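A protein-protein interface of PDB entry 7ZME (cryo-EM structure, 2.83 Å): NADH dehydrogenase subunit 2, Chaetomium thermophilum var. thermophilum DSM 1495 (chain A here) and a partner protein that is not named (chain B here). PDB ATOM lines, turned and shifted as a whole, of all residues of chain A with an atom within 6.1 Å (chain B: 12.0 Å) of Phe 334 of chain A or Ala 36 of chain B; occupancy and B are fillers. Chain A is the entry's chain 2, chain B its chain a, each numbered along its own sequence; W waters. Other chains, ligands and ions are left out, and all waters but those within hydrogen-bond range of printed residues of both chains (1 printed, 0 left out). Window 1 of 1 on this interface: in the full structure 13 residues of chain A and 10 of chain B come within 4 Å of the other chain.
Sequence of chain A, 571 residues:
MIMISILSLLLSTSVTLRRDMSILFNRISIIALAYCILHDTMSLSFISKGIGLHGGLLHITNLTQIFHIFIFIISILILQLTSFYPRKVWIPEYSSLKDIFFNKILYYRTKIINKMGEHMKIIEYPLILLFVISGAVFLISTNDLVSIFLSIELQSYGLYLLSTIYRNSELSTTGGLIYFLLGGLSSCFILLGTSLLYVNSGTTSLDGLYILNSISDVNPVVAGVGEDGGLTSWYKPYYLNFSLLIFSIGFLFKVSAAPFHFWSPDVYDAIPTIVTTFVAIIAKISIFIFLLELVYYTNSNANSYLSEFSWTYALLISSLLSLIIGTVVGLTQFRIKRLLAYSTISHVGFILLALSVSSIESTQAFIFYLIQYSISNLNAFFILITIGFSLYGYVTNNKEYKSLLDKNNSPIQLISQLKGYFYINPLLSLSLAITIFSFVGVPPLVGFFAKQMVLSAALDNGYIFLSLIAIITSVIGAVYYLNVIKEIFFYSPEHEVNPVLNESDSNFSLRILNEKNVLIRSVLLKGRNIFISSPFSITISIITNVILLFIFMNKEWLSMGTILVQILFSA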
ATOM      1  N   THR A 332     -21.954 -17.409  34.577  1.00  0.00           N
ATOM      2  CA  THR A 332     -22.037 -18.251  33.391  1.00  0.00           C
ATOM      3  C   THR A 332     -22.390 -17.463  32.138  1.00  0.00           C
ATOM      4  O   THR A 332     -22.936 -18.030  31.190  1.00  0.00           O
ATOM      5  CB  THR A 332     -23.051 -19.376  33.600  1.00  0.00           C
ATOM      6  OG1 THR A 332     -24.245 -18.844  34.183  1.00  0.00           O
ATOM      7  CG2 THR A 332     -22.477 -20.448  34.501  1.00  0.00           C
ATOM      8  N   GLN A 333     -22.048 -16.183  32.100  1.00  0.00           N
ATOM      9  CA  GLN A 333     -22.276 -15.363  30.879  1.00  0.00           C
ATOM     10  C   GLN A 333     -21.059 -15.466  29.953  1.00  0.00           C
ATOM     11  O   GLN A 333     -19.959 -15.125  30.400  1.00  0.00           O
ATOM     12  CB  GLN A 333     -22.573 -13.917  31.278  1.00  0.00           C
ATOM     13  CG  GLN A 333     -23.850 -13.753  32.086  1.00  0.00           C
ATOM     14  CD  GLN A 333     -25.086 -14.211  31.351  1.00  0.00           C
ATOM     15  OE1 GLN A 333     -25.491 -13.618  30.356  1.00  0.00           O
ATOM     16  NE2 GLN A 333     -25.707 -15.268  31.848  1.00  0.00           N
ATOM     17  N   PHE A 334     -21.251 -15.947  28.725  1.00  0.00           N
ATOM     18  CA  PHE A 334     -20.138 -16.116  27.758  1.00  0.00           C
ATOM     19  C   PHE A 334     -20.129 -14.921  26.815  1.00  0.00           C
ATOM     20  O   PHE A 334     -19.148 -14.712  26.093  1.00  0.00           O
ATOM     21  CB  PHE A 334     -20.297 -17.438  27.009  1.00  0.00           C
ATOM     22  CG  PHE A 334     -21.506 -17.564  26.120  1.00  0.00           C
ATOM     23  CD1 PHE A 334     -22.742 -17.904  26.643  1.00  0.00           C
ATOM     24  CD2 PHE A 334     -21.396 -17.397  24.749  1.00  0.00           C
ATOM     25  CE1 PHE A 334     -23.849 -18.034  25.821  1.00  0.00           C
ATOM     26  CE2 PHE A 334     -22.503 -17.531  23.929  1.00  0.00           C
ATOM     27  CZ  PHE A 334     -23.727 -17.844  24.467  1.00  0.00           C
ATOM     28  N   ARG A 335     -21.210 -14.152  26.838  1.00  0.00           N
ATOM     29  CA  ARG A 335     -21.328 -12.980  25.937  1.00  0.00           C
ATOM     30  C   ARG A 335     -20.807 -11.749  26.683  1.00  0.00           C
ATOM     31  O   ARG A 335     -21.287 -11.503  27.788  1.00  0.00           O
ATOM     32  CB  ARG A 335     -22.731 -12.955  25.329  1.00  0.00           C
ATOM     33  CG  ARG A 335     -22.976 -14.084  24.345  1.00  0.00           C
ATOM     34  CD  ARG A 335     -24.273 -13.964  23.576  1.00  0.00           C
ATOM     35  NE  ARG A 335     -24.360 -12.700  22.869  1.00  0.00           N
ATOM     36  CZ  ARG A 335     -23.908 -12.476  21.642  1.00  0.00           C
ATOM     37  NH1 ARG A 335     -24.047 -11.282  21.100  1.00  0.00           N
ATOM     38  NH2 ARG A 335     -23.320 -13.443  20.965  1.00  0.00           N
ATOM     39  N   ILE A 336     -19.868 -11.016  26.090  1.00  0.00           N
ATOM     40  CA  ILE A 336     -19.194  -9.868  26.769  1.00  0.00           C
ATOM     41  C   ILE A 336     -20.202  -8.790  27.186  1.00  0.00           C
ATOM     42  O   ILE A 336     -20.068  -8.279  28.300  1.00  0.00           O
ATOM     43  CB  ILE A 336     -18.066  -9.302  25.875  1.00  0.00           C
ATOM     44  CG1 ILE A 336     -17.209  -8.273  26.618  1.00  0.00           C
ATOM     45  CG2 ILE A 336     -18.583  -8.760  24.553  1.00  0.00           C
ATOM     46  CD1 ILE A 336     -16.497  -8.824  27.832  1.00  0.00           C
ATOM     47  N   ARG A 338     -23.518  -9.248  27.589  1.00  0.00           N
ATOM     48  CA  ARG A 338     -24.503  -9.811  28.541  1.00  0.00           C
ATOM     49  C   ARG A 338     -23.831  -9.761  29.911  1.00  0.00           C
ATOM     50  O   ARG A 338     -24.543  -9.728  30.923  1.00  0.00           O
ATOM     51  CB  ARG A 338     -24.962 -11.203  28.096  1.00  0.00           C
ATOM     52  CG  ARG A 338     -26.070 -11.199  27.060  1.00  0.00           C
ATOM     53  CD  ARG A 338     -26.779 -12.534  27.009  1.00  0.00           C
ATOM     54  NE  ARG A 338     -27.505 -12.794  28.242  1.00  0.00           N
ATOM     55  CZ  ARG A 338     -28.786 -12.508  28.436  1.00  0.00           C
ATOM     56  NH1 ARG A 338     -29.492 -11.952  27.468  1.00  0.00           N
ATOM     57  NH2 ARG A 338     -29.354 -12.781  29.595  1.00  0.00           N
ATOM     58  N   GLN A 413     -18.514  -9.913  20.572  1.00  0.00           N
ATOM     59  CA  GLN A 413     -19.773 -10.352  21.214  1.00  0.00           C
ATOM     60  C   GLN A 413     -19.445 -11.452  22.210  1.00  0.00           C
ATOM     61  O   GLN A 413     -20.322 -11.810  22.999  1.00  0.00           O
ATOM     62  CB  GLN A 413     -20.709 -10.924  20.147  1.00  0.00           C
ATOM     63  CG  GLN A 413     -20.839 -10.062  18.907  1.00  0.00           C
ATOM     64  CD  GLN A 413     -21.971 -10.493  18.011  1.00  0.00           C
ATOM     65  OE1 GLN A 413     -22.883 -11.194  18.429  1.00  0.00           O
ATOM     66  NE2 GLN A 413     -21.921 -10.066  16.762  1.00  0.00           N
ATOM     67  N   LEU A 414     -18.213 -11.946  22.172  1.00  0.00           N
ATOM     68  CA  LEU A 414     -17.853 -13.100  23.026  1.00  0.00           C
ATOM     69  C   LEU A 414     -16.636 -12.751  23.866  1.00  0.00           C
ATOM     70  O   LEU A 414     -15.804 -11.968  23.394  1.00  0.00           O
ATOM     71  CB  LEU A 414     -17.546 -14.305  22.135  1.00  0.00           C
ATOM     72  CG  LEU A 414     -18.692 -14.801  21.258  1.00  0.00           C
ATOM     73  CD1 LEU A 414     -18.200 -15.860  20.289  1.00  0.00           C
ATOM     74  CD2 LEU A 414     -19.828 -15.345  22.107  1.00  0.00           C
ATOM     75  N   ILE A 415     -16.566 -13.289  25.080  1.00  0.00           N
ATOM     76  CA  ILE A 415     -15.345 -13.112  25.916  1.00  0.00           C
ATOM     77  C   ILE A 415     -14.206 -13.867  25.230  1.00  0.00           C
ATOM     78  O   ILE A 415     -13.087 -13.356  25.229  1.00  0.00           O
ATOM     79  CB  ILE A 415     -15.628 -13.586  27.356  1.00  0.00           C
ATOM     80  CG1 ILE A 415     -16.817 -12.819  27.941  1.00  0.00           C
ATOM     81  CG2 ILE A 415     -14.394 -13.467  28.235  1.00  0.00           C
ATOM     82  CD1 ILE A 415     -17.305 -13.332  29.265  1.00  0.00           C
ATOM     83  N   SER A 416     -14.496 -15.018  24.632  1.00  0.00           N
ATOM     84  CA  SER A 416     -13.475 -15.865  23.964  1.00  0.00           C
ATOM     85  C   SER A 416     -12.858 -15.146  22.769  1.00  0.00           C
ATOM     86  O   SER A 416     -11.778 -15.557  22.351  1.00  0.00           O
ATOM     87  CB  SER A 416     -14.071 -17.166  23.538  1.00  0.00           C
ATOM     88  OG  SER A 416     -15.095 -16.966  22.579  1.00  0.00           O
ATOM     89  N   PHE B  32     -37.973 -13.500  21.317  1.00  0.00           N
ATOM     90  CA  PHE B  32     -37.807 -12.748  20.050  1.00  0.00           C
ATOM     91  C   PHE B  32     -36.330 -12.734  19.661  1.00  0.00           C
ATOM     92  O   PHE B  32     -36.029 -12.674  18.457  1.00  0.00           O
ATOM     93  CB  PHE B  32     -38.391 -11.340  20.179  1.00  0.00           C
ATOM     94  CG  PHE B  32     -39.895 -11.260  20.185  1.00  0.00           C
ATOM     95  CD1 PHE B  32     -40.645 -11.931  19.233  1.00  0.00           C
ATOM     96  CD2 PHE B  32     -40.560 -10.497  21.129  1.00  0.00           C
ATOM     97  CE1 PHE B  32     -42.029 -11.855  19.237  1.00  0.00           C
ATOM     98  CE2 PHE B  32     -41.944 -10.418  21.129  1.00  0.00           C
ATOM     99  CZ  PHE B  32     -42.675 -11.097  20.182  1.00  0.00           C
ATOM    100  N   LEU B  33     -35.439 -12.781  20.652  1.00  0.00           N
ATOM    101  CA  LEU B  33     -33.981 -12.796  20.367  1.00  0.00           C
ATOM    102  C   LEU B  33     -33.524 -14.174  19.877  1.00  0.00           C
ATOM    103  O   LEU B  33     -34.212 -15.161  20.169  1.00  0.00           O
ATOM    104  CB  LEU B  33     -33.204 -12.341  21.601  1.00  0.00           C
ATOM    105  CG  LEU B  33     -33.009 -10.836  21.759  1.00  0.00           C
ATOM    106  CD1 LEU B  33     -32.048 -10.543  22.897  1.00  0.00           C
ATOM    107  CD2 LEU B  33     -32.493 -10.217  20.477  1.00  0.00           C
ATOM    108  N   PRO B  34     -32.384 -14.278  19.159  1.00  0.00           N
ATOM    109  CA  PRO B  34     -31.853 -15.560  18.667  1.00  0.00           C
ATOM    110  C   PRO B  34     -31.442 -16.575  19.740  1.00  0.00           C
ATOM    111  O   PRO B  34     -31.077 -16.159  20.816  1.00  0.00           O
ATOM    112  CB  PRO B  34     -30.605 -15.149  17.875  1.00  0.00           C
ATOM    113  CG  PRO B  34     -30.883 -13.729  17.471  1.00  0.00           C
ATOM    114  CD  PRO B  34     -31.571 -13.161  18.688  1.00  0.00           C
ATOM    115  N   GLU B  35     -31.480 -17.870  19.415  1.00  0.00           N
ATOM    116  CA  GLU B  35     -31.231 -18.936  20.431  1.00  0.00           C
ATOM    117  C   GLU B  35     -29.833 -18.857  21.065  1.00  0.00           C
ATOM    118  O   GLU B  35     -29.752 -19.055  22.270  1.00  0.00           O
ATOM    119  CB  GLU B  35     -31.483 -20.316  19.826  1.00  0.00           C
ATOM    120  CG  GLU B  35     -32.952 -20.694  19.783  1.00  0.00           C
ATOM    121  CD  GLU B  35     -33.555 -21.047  21.133  1.00  0.00           C
ATOM    122  OE1 GLU B  35     -32.784 -21.354  22.065  1.00  0.00           O
ATOM    123  OE2 GLU B  35     -34.796 -21.013  21.248  1.00  0.00           O
ATOM    124  N   ALA B  36     -28.756 -18.658  20.299  1.00  0.00           N
ATOM    125  CA  ALA B  36     -27.436 -18.547  20.968  1.00  0.00           C
ATOM    126  C   ALA B  36     -27.362 -17.427  22.009  1.00  0.00           C
ATOM    127  O   ALA B  36     -26.805 -17.679  23.089  1.00  0.00           O
ATOM    128  CB  ALA B  36     -26.363 -18.391  19.931  1.00  0.00           C
ATOM    129  N   MET B  37     -27.898 -16.246  21.700  1.00  0.00           N
ATOM    130  CA  MET B  37     -27.756 -15.060  22.583  1.00  0.00           C
ATOM    131  C   MET B  37     -28.411 -15.223  23.957  1.00  0.00           C
ATOM    132  O   MET B  37     -27.844 -14.710  24.921  1.00  0.00           O
ATOM    133  CB  MET B  37     -28.241 -13.802  21.868  1.00  0.00           C
ATOM    134  CG  MET B  37     -27.337 -13.411  20.726  1.00  0.00           C
ATOM    135  SD  MET B  37     -27.973 -12.028  19.772  1.00  0.00           S
ATOM    136  CE  MET B  37     -28.303 -10.840  21.071  1.00  0.00           C
ATOM    137  N   VAL B  38     -29.519 -15.905  24.068  1.00  0.00           N
ATOM    138  CA  VAL B  38     -30.232 -15.991  25.376  1.00  0.00           C
ATOM    139  C   VAL B  38     -30.548 -17.467  25.682  1.00  0.00           C
ATOM    140  O   VAL B  38     -31.228 -17.740  26.678  1.00  0.00           O
ATOM    141  CB  VAL B  38     -31.485 -15.089  25.351  1.00  0.00           C
ATOM    142  CG1 VAL B  38     -32.534 -15.573  24.365  1.00  0.00           C
ATOM    143  CG2 VAL B  38     -32.076 -14.852  26.728  1.00  0.00           C
ATOM    144  N   GLY B  39     -30.086 -18.391  24.841  1.00  0.00           N
ATOM    145  CA  GLY B  39     -30.399 -19.817  25.078  1.00  0.00           C
ATOM    146  C   GLY B  39     -29.609 -20.437  26.214  1.00  0.00           C
ATOM    147  O   GLY B  39     -28.432 -20.075  26.389  1.00  0.00           O
ATOM    148  N   ARG B  40     -30.233 -21.356  26.950  1.00  0.00           N
ATOM    149  CA  ARG B  40     -29.532 -22.050  28.060  1.00  0.00           C
ATOM    150  C   ARG B  40     -28.632 -23.125  27.458  1.00  0.00           C
ATOM    151  O   ARG B  40     -27.595 -23.406  28.054  1.00  0.00           O
ATOM    152  CB  ARG B  40     -30.538 -22.676  29.032  1.00  0.00           C
ATOM    153  CG  ARG B  40     -29.934 -23.049  30.379  1.00  0.00           C
ATOM    154  CD  ARG B  40     -30.877 -23.814  31.289  1.00  0.00           C
ATOM    155  NE  ARG B  40     -30.293 -24.015  32.607  1.00  0.00           N
ATOM    156  CZ  ARG B  40     -29.593 -25.086  32.965  1.00  0.00           C
ATOM    157  NH1 ARG B  40     -29.398 -26.069  32.103  1.00  0.00           N
ATOM    158  NH2 ARG B  40     -29.097 -25.176  34.185  1.00  0.00           N
ATOM    159  N   SER B  41     -29.026 -23.678  26.313  1.00  0.00           N
ATOM    160  CA  SER B  41     -28.238 -24.746  25.654  1.00  0.00           C
ATOM    161  C   SER B  41     -26.851 -24.251  25.256  1.00  0.00           C
ATOM    162  O   SER B  41     -25.906 -25.044  25.371  1.00  0.00           O
ATOM    163  CB  SER B  41     -28.980 -25.291  24.466  1.00  0.00           C
ATOM    164  OG  SER B  41     -29.306 -24.255  23.549  1.00  0.00           O
ATOM    165  N   LYS B  42     -26.732 -23.022  24.764  1.00  0.00           N
ATOM    166  CA  LYS B  42     -25.388 -22.464  24.460  1.00  0.00           C
ATOM    167  C   LYS B  42     -24.583 -22.335  25.757  1.00  0.00           C
ATOM    168  O   LYS B  42     -23.385 -22.594  25.704  1.00  0.00           O
ATOM    169  CB  LYS B  42     -25.504 -21.174  23.644  1.00  0.00           C
ATOM    170  CG  LYS B  42     -24.303 -20.861  22.763  1.00  0.00           C
ATOM    171  CD  LYS B  42     -24.072 -21.899  21.690  1.00  0.00           C
ATOM    172  CE  LYS B  42     -22.833 -21.623  20.864  1.00  0.00           C
ATOM    173  NZ  LYS B  42     -21.599 -21.741  21.674  1.00  0.00           N
ATOM    174  N   ILE B  43     -25.215 -21.924  26.861  1.00  0.00           N
ATOM    175  CA  ILE B  43     -24.524 -21.863  28.183  1.00  0.00           C
ATOM    176  C   ILE B  43     -24.132 -23.283  28.571  1.00  0.00           C
ATOM    177  O   ILE B  43     -23.041 -23.463  29.108  1.00  0.00           O
ATOM    178  CB  ILE B  43     -25.444 -21.234  29.246  1.00  0.00           C
ATOM    179  CG1 ILE B  43     -26.109 -19.950  28.743  1.00  0.00           C
ATOM    180  CG2 ILE B  43     -24.710 -21.012  30.557  1.00  0.00           C
ATOM    181  CD1 ILE B  43     -25.366 -18.687  29.104  1.00  0.00           C
ATOM    182  N   ASP B  44     -25.017 -24.246  28.317  1.00  0.00           N
ATOM    183  CA  ASP B  44     -24.748 -25.671  28.628  1.00  0.00           C
ATOM    184  C   ASP B  44     -23.559 -26.146  27.789  1.00  0.00           C
ATOM    185  O   ASP B  44     -22.851 -27.047  28.247  1.00  0.00           O
ATOM    186  CB  ASP B  44     -26.038 -26.482  28.528  1.00  0.00           C
ATOM    187  CG  ASP B  44     -27.039 -26.120  29.606  1.00  0.00           C
ATOM    188  OD1 ASP B  44     -26.616 -25.515  30.607  1.00  0.00           O
ATOM    189  OD2 ASP B  44     -28.232 -26.437  29.431  1.00  0.00           O
ATOM    190  N   GLU B  45     -23.361 -25.591  26.593  1.00  0.00           N
ATOM    191  CA  GLU B  45     -22.153 -25.909  25.846  1.00  0.00           C
ATOM    192  C   GLU B  45     -20.936 -25.235  26.466  1.00  0.00           C
ATOM    193  O   GLU B  45     -19.863 -25.842  26.559  1.00  0.00           O
ATOM    194  CB  GLU B  45     -22.313 -25.498  24.383  1.00  0.00           C
ATOM    195  CG  GLU B  45     -21.125 -25.867  23.506  1.00  0.00           C
ATOM    196  CD  GLU B  45     -21.332 -25.494  22.053  1.00  0.00           C
ATOM    197  OE1 GLU B  45     -22.396 -24.926  21.728  1.00  0.00           O
ATOM    198  OE2 GLU B  45     -20.429 -25.767  21.233  1.00  0.00           O
ATOM    199  N   LYS B  46     -21.088 -23.982  26.900  1.00  0.00           N
ATOM    200  CA  LYS B  46     -19.975 -23.255  27.497  1.00  0.00           C
ATOM    201  C   LYS B  46     -19.609 -23.809  28.865  1.00  0.00           C
ATOM    202  O   LYS B  46     -18.432 -23.809  29.241  1.00  0.00           O
ATOM    203  CB  LYS B  46     -20.320 -21.769  27.601  1.00  0.00           C
ATOM    204  CG  LYS B  46     -20.615 -21.059  26.278  1.00  0.00           C
ATOM    205  CD  LYS B  46     -19.374 -20.866  25.406  1.00  0.00           C
ATOM    206  CE  LYS B  46     -19.180 -21.985  24.391  1.00  0.00           C
ATOM    207  NZ  LYS B  46     -18.028 -21.717  23.488  1.00  0.00           N
ATOM    208  N   TYR B  47     -20.597 -24.276  29.623  1.00  0.00           N
ATOM    209  CA  TYR B  47     -20.387 -24.849  30.951  1.00  0.00           C
ATOM    210  C   TYR B  47     -21.147 -26.165  31.027  1.00  0.00           C
ATOM    211  O   TYR B  47     -22.254 -26.226  31.576  1.00  0.00           O
ATOM    212  CB  TYR B  47     -20.833 -23.881  32.048  1.00  0.00           C
ATOM    213  CG  TYR B  47     -20.324 -22.474  31.855  1.00  0.00           C
ATOM    214  CD1 TYR B  47     -19.110 -22.074  32.391  1.00  0.00           C
ATOM    215  CD2 TYR B  47     -21.057 -21.546  31.136  1.00  0.00           C
ATOM    216  CE1 TYR B  47     -18.643 -20.795  32.216  1.00  0.00           C
ATOM    217  CE2 TYR B  47     -20.595 -20.266  30.953  1.00  0.00           C
ATOM    218  CZ  TYR B  47     -19.389 -19.894  31.499  1.00  0.00           C
ATOM    219  OH  TYR B  47     -18.929 -18.611  31.318  1.00  0.00           O
ATOM    220  N   PRO B  48     -20.592 -27.236  30.463  1.00  0.00           N
ATOM    221  CA  PRO B  48     -21.239 -28.545  30.579  1.00  0.00           C
ATOM    222  C   PRO B  48     -21.242 -29.045  32.013  1.00  0.00           C
ATOM    223  O   PRO B  48     -20.347 -28.748  32.805  1.00  0.00           O
ATOM    224  CB  PRO B  48     -20.383 -29.445  29.682  1.00  0.00           C
ATOM    225  CG  PRO B  48     -19.658 -28.507  28.772  1.00  0.00           C
ATOM    226  CD  PRO B  48     -19.419 -27.276  29.576  1.00  0.00           C
HETATM  227  O   HOH W   1     -27.415 -15.983  27.930  1.00  0.00           O
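Gln 333 of chain A touches just one residue of chain B: Tyr 47. Ile 336 of chain A touches none of the printed residues of chain B. Printed residues of chain B within 4 Å of Arg 338 of chain A: Met 37 (3.2 Å) and Val 38 (3.95 Å). No residue of chain B comes within 4 Å of Ile 415 of chain A. Ser 416 of chain A touches none of the printed residues of chain B. Of the printed residues of chain A, Ala 36 of chain B touches Phe 334 (3.4 Å). Printed residues of chain A within 4 Å of Met 37 of chain B: Arg 335 and Arg 338. Of the printed residues of chain A, Lys 46 of chain B touches Phe 334. The nearest residue of chain B that does not touch Phe 334 of chain A is Tyr 47 of chain B (4.4 Å). The nearest residue of chain A that does not touch Ala 36 of chain B is Arg 335 of chain A (4.5 Å). The nearest printed residue of chain A that does not touch Met 37 of chain B is Phe 334 of chain A (5.2 Å).
Water W1 lies within hydrogen-bond range of NE of Arg 338 of chain A and O of Met 37 of chain B.
Of the 10 printed residues of chain A, 5 touch a printed residue of chain B. Printed residues of chain A that touch a printed residue of chain B: Thr 332, Gln 333, Phe 334, Arg 335 and Arg 338. Hydrophobic or aromatic side chains of chain A within 4 Å of the printed part of chain B: Phe 334. Of the 17 printed residues of chain B, 7 touch a printed residue of chain A. Hydrophobic or aromatic side chains of chain B that line the printed part of chain A: Met 37, Val 38, Ile 43 and Tyr 47. Among the printed residues, 10 pairs touch across the chains. Among the printed residues, no Asp or Glu carboxylate lies within 4 Å of a Lys or Arg side-chain nitrogen of the other chain.
O of Phe 334 of chain A lies within hydrogen-bond range of N of Ile 415 of chain A (3.1 Å). OE1 of Gln 333 of chain A sits at hydrogen-bond distance from NE of Arg 338 of chain A. NH1 of Arg 335 of chain A lies within hydrogen-bond range of OE1 of Gln 413 of chain A. The side-chain amino group (NZ) of Lys 42 of chain B lies within salt-bridge range of the side-chain carboxylate (OE1) of Glu 45 of chain B (3.3 Å).
O of Thr 332 of chain A touches CD1 of Ile 43 of chain B, 3.3 Å away. O of Thr 332 of chain A touches CE2 of Tyr 47 of chain B, at 3.2 Å. Gln 333 of chain A touches Tyr 47 of chain B. O of Ala 36 of chain B touches CZ of Phe 334 of chain A (3.4 Å). Lys 42 of chain B touches Phe 334 of chain A. Ile 43 of chain B touches Phe 334 of chain A. Lys 46 of chain B touches Phe 334 of chain A. CZ of Arg 335 of chain A touches CG of Met 37 of chain B, at 3.7 Å. Arg 338 of chain A touches Met 37 of chain B (CD to O, 3.2 Å). Arg 338 of chain A touches Val 38 of chain B.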
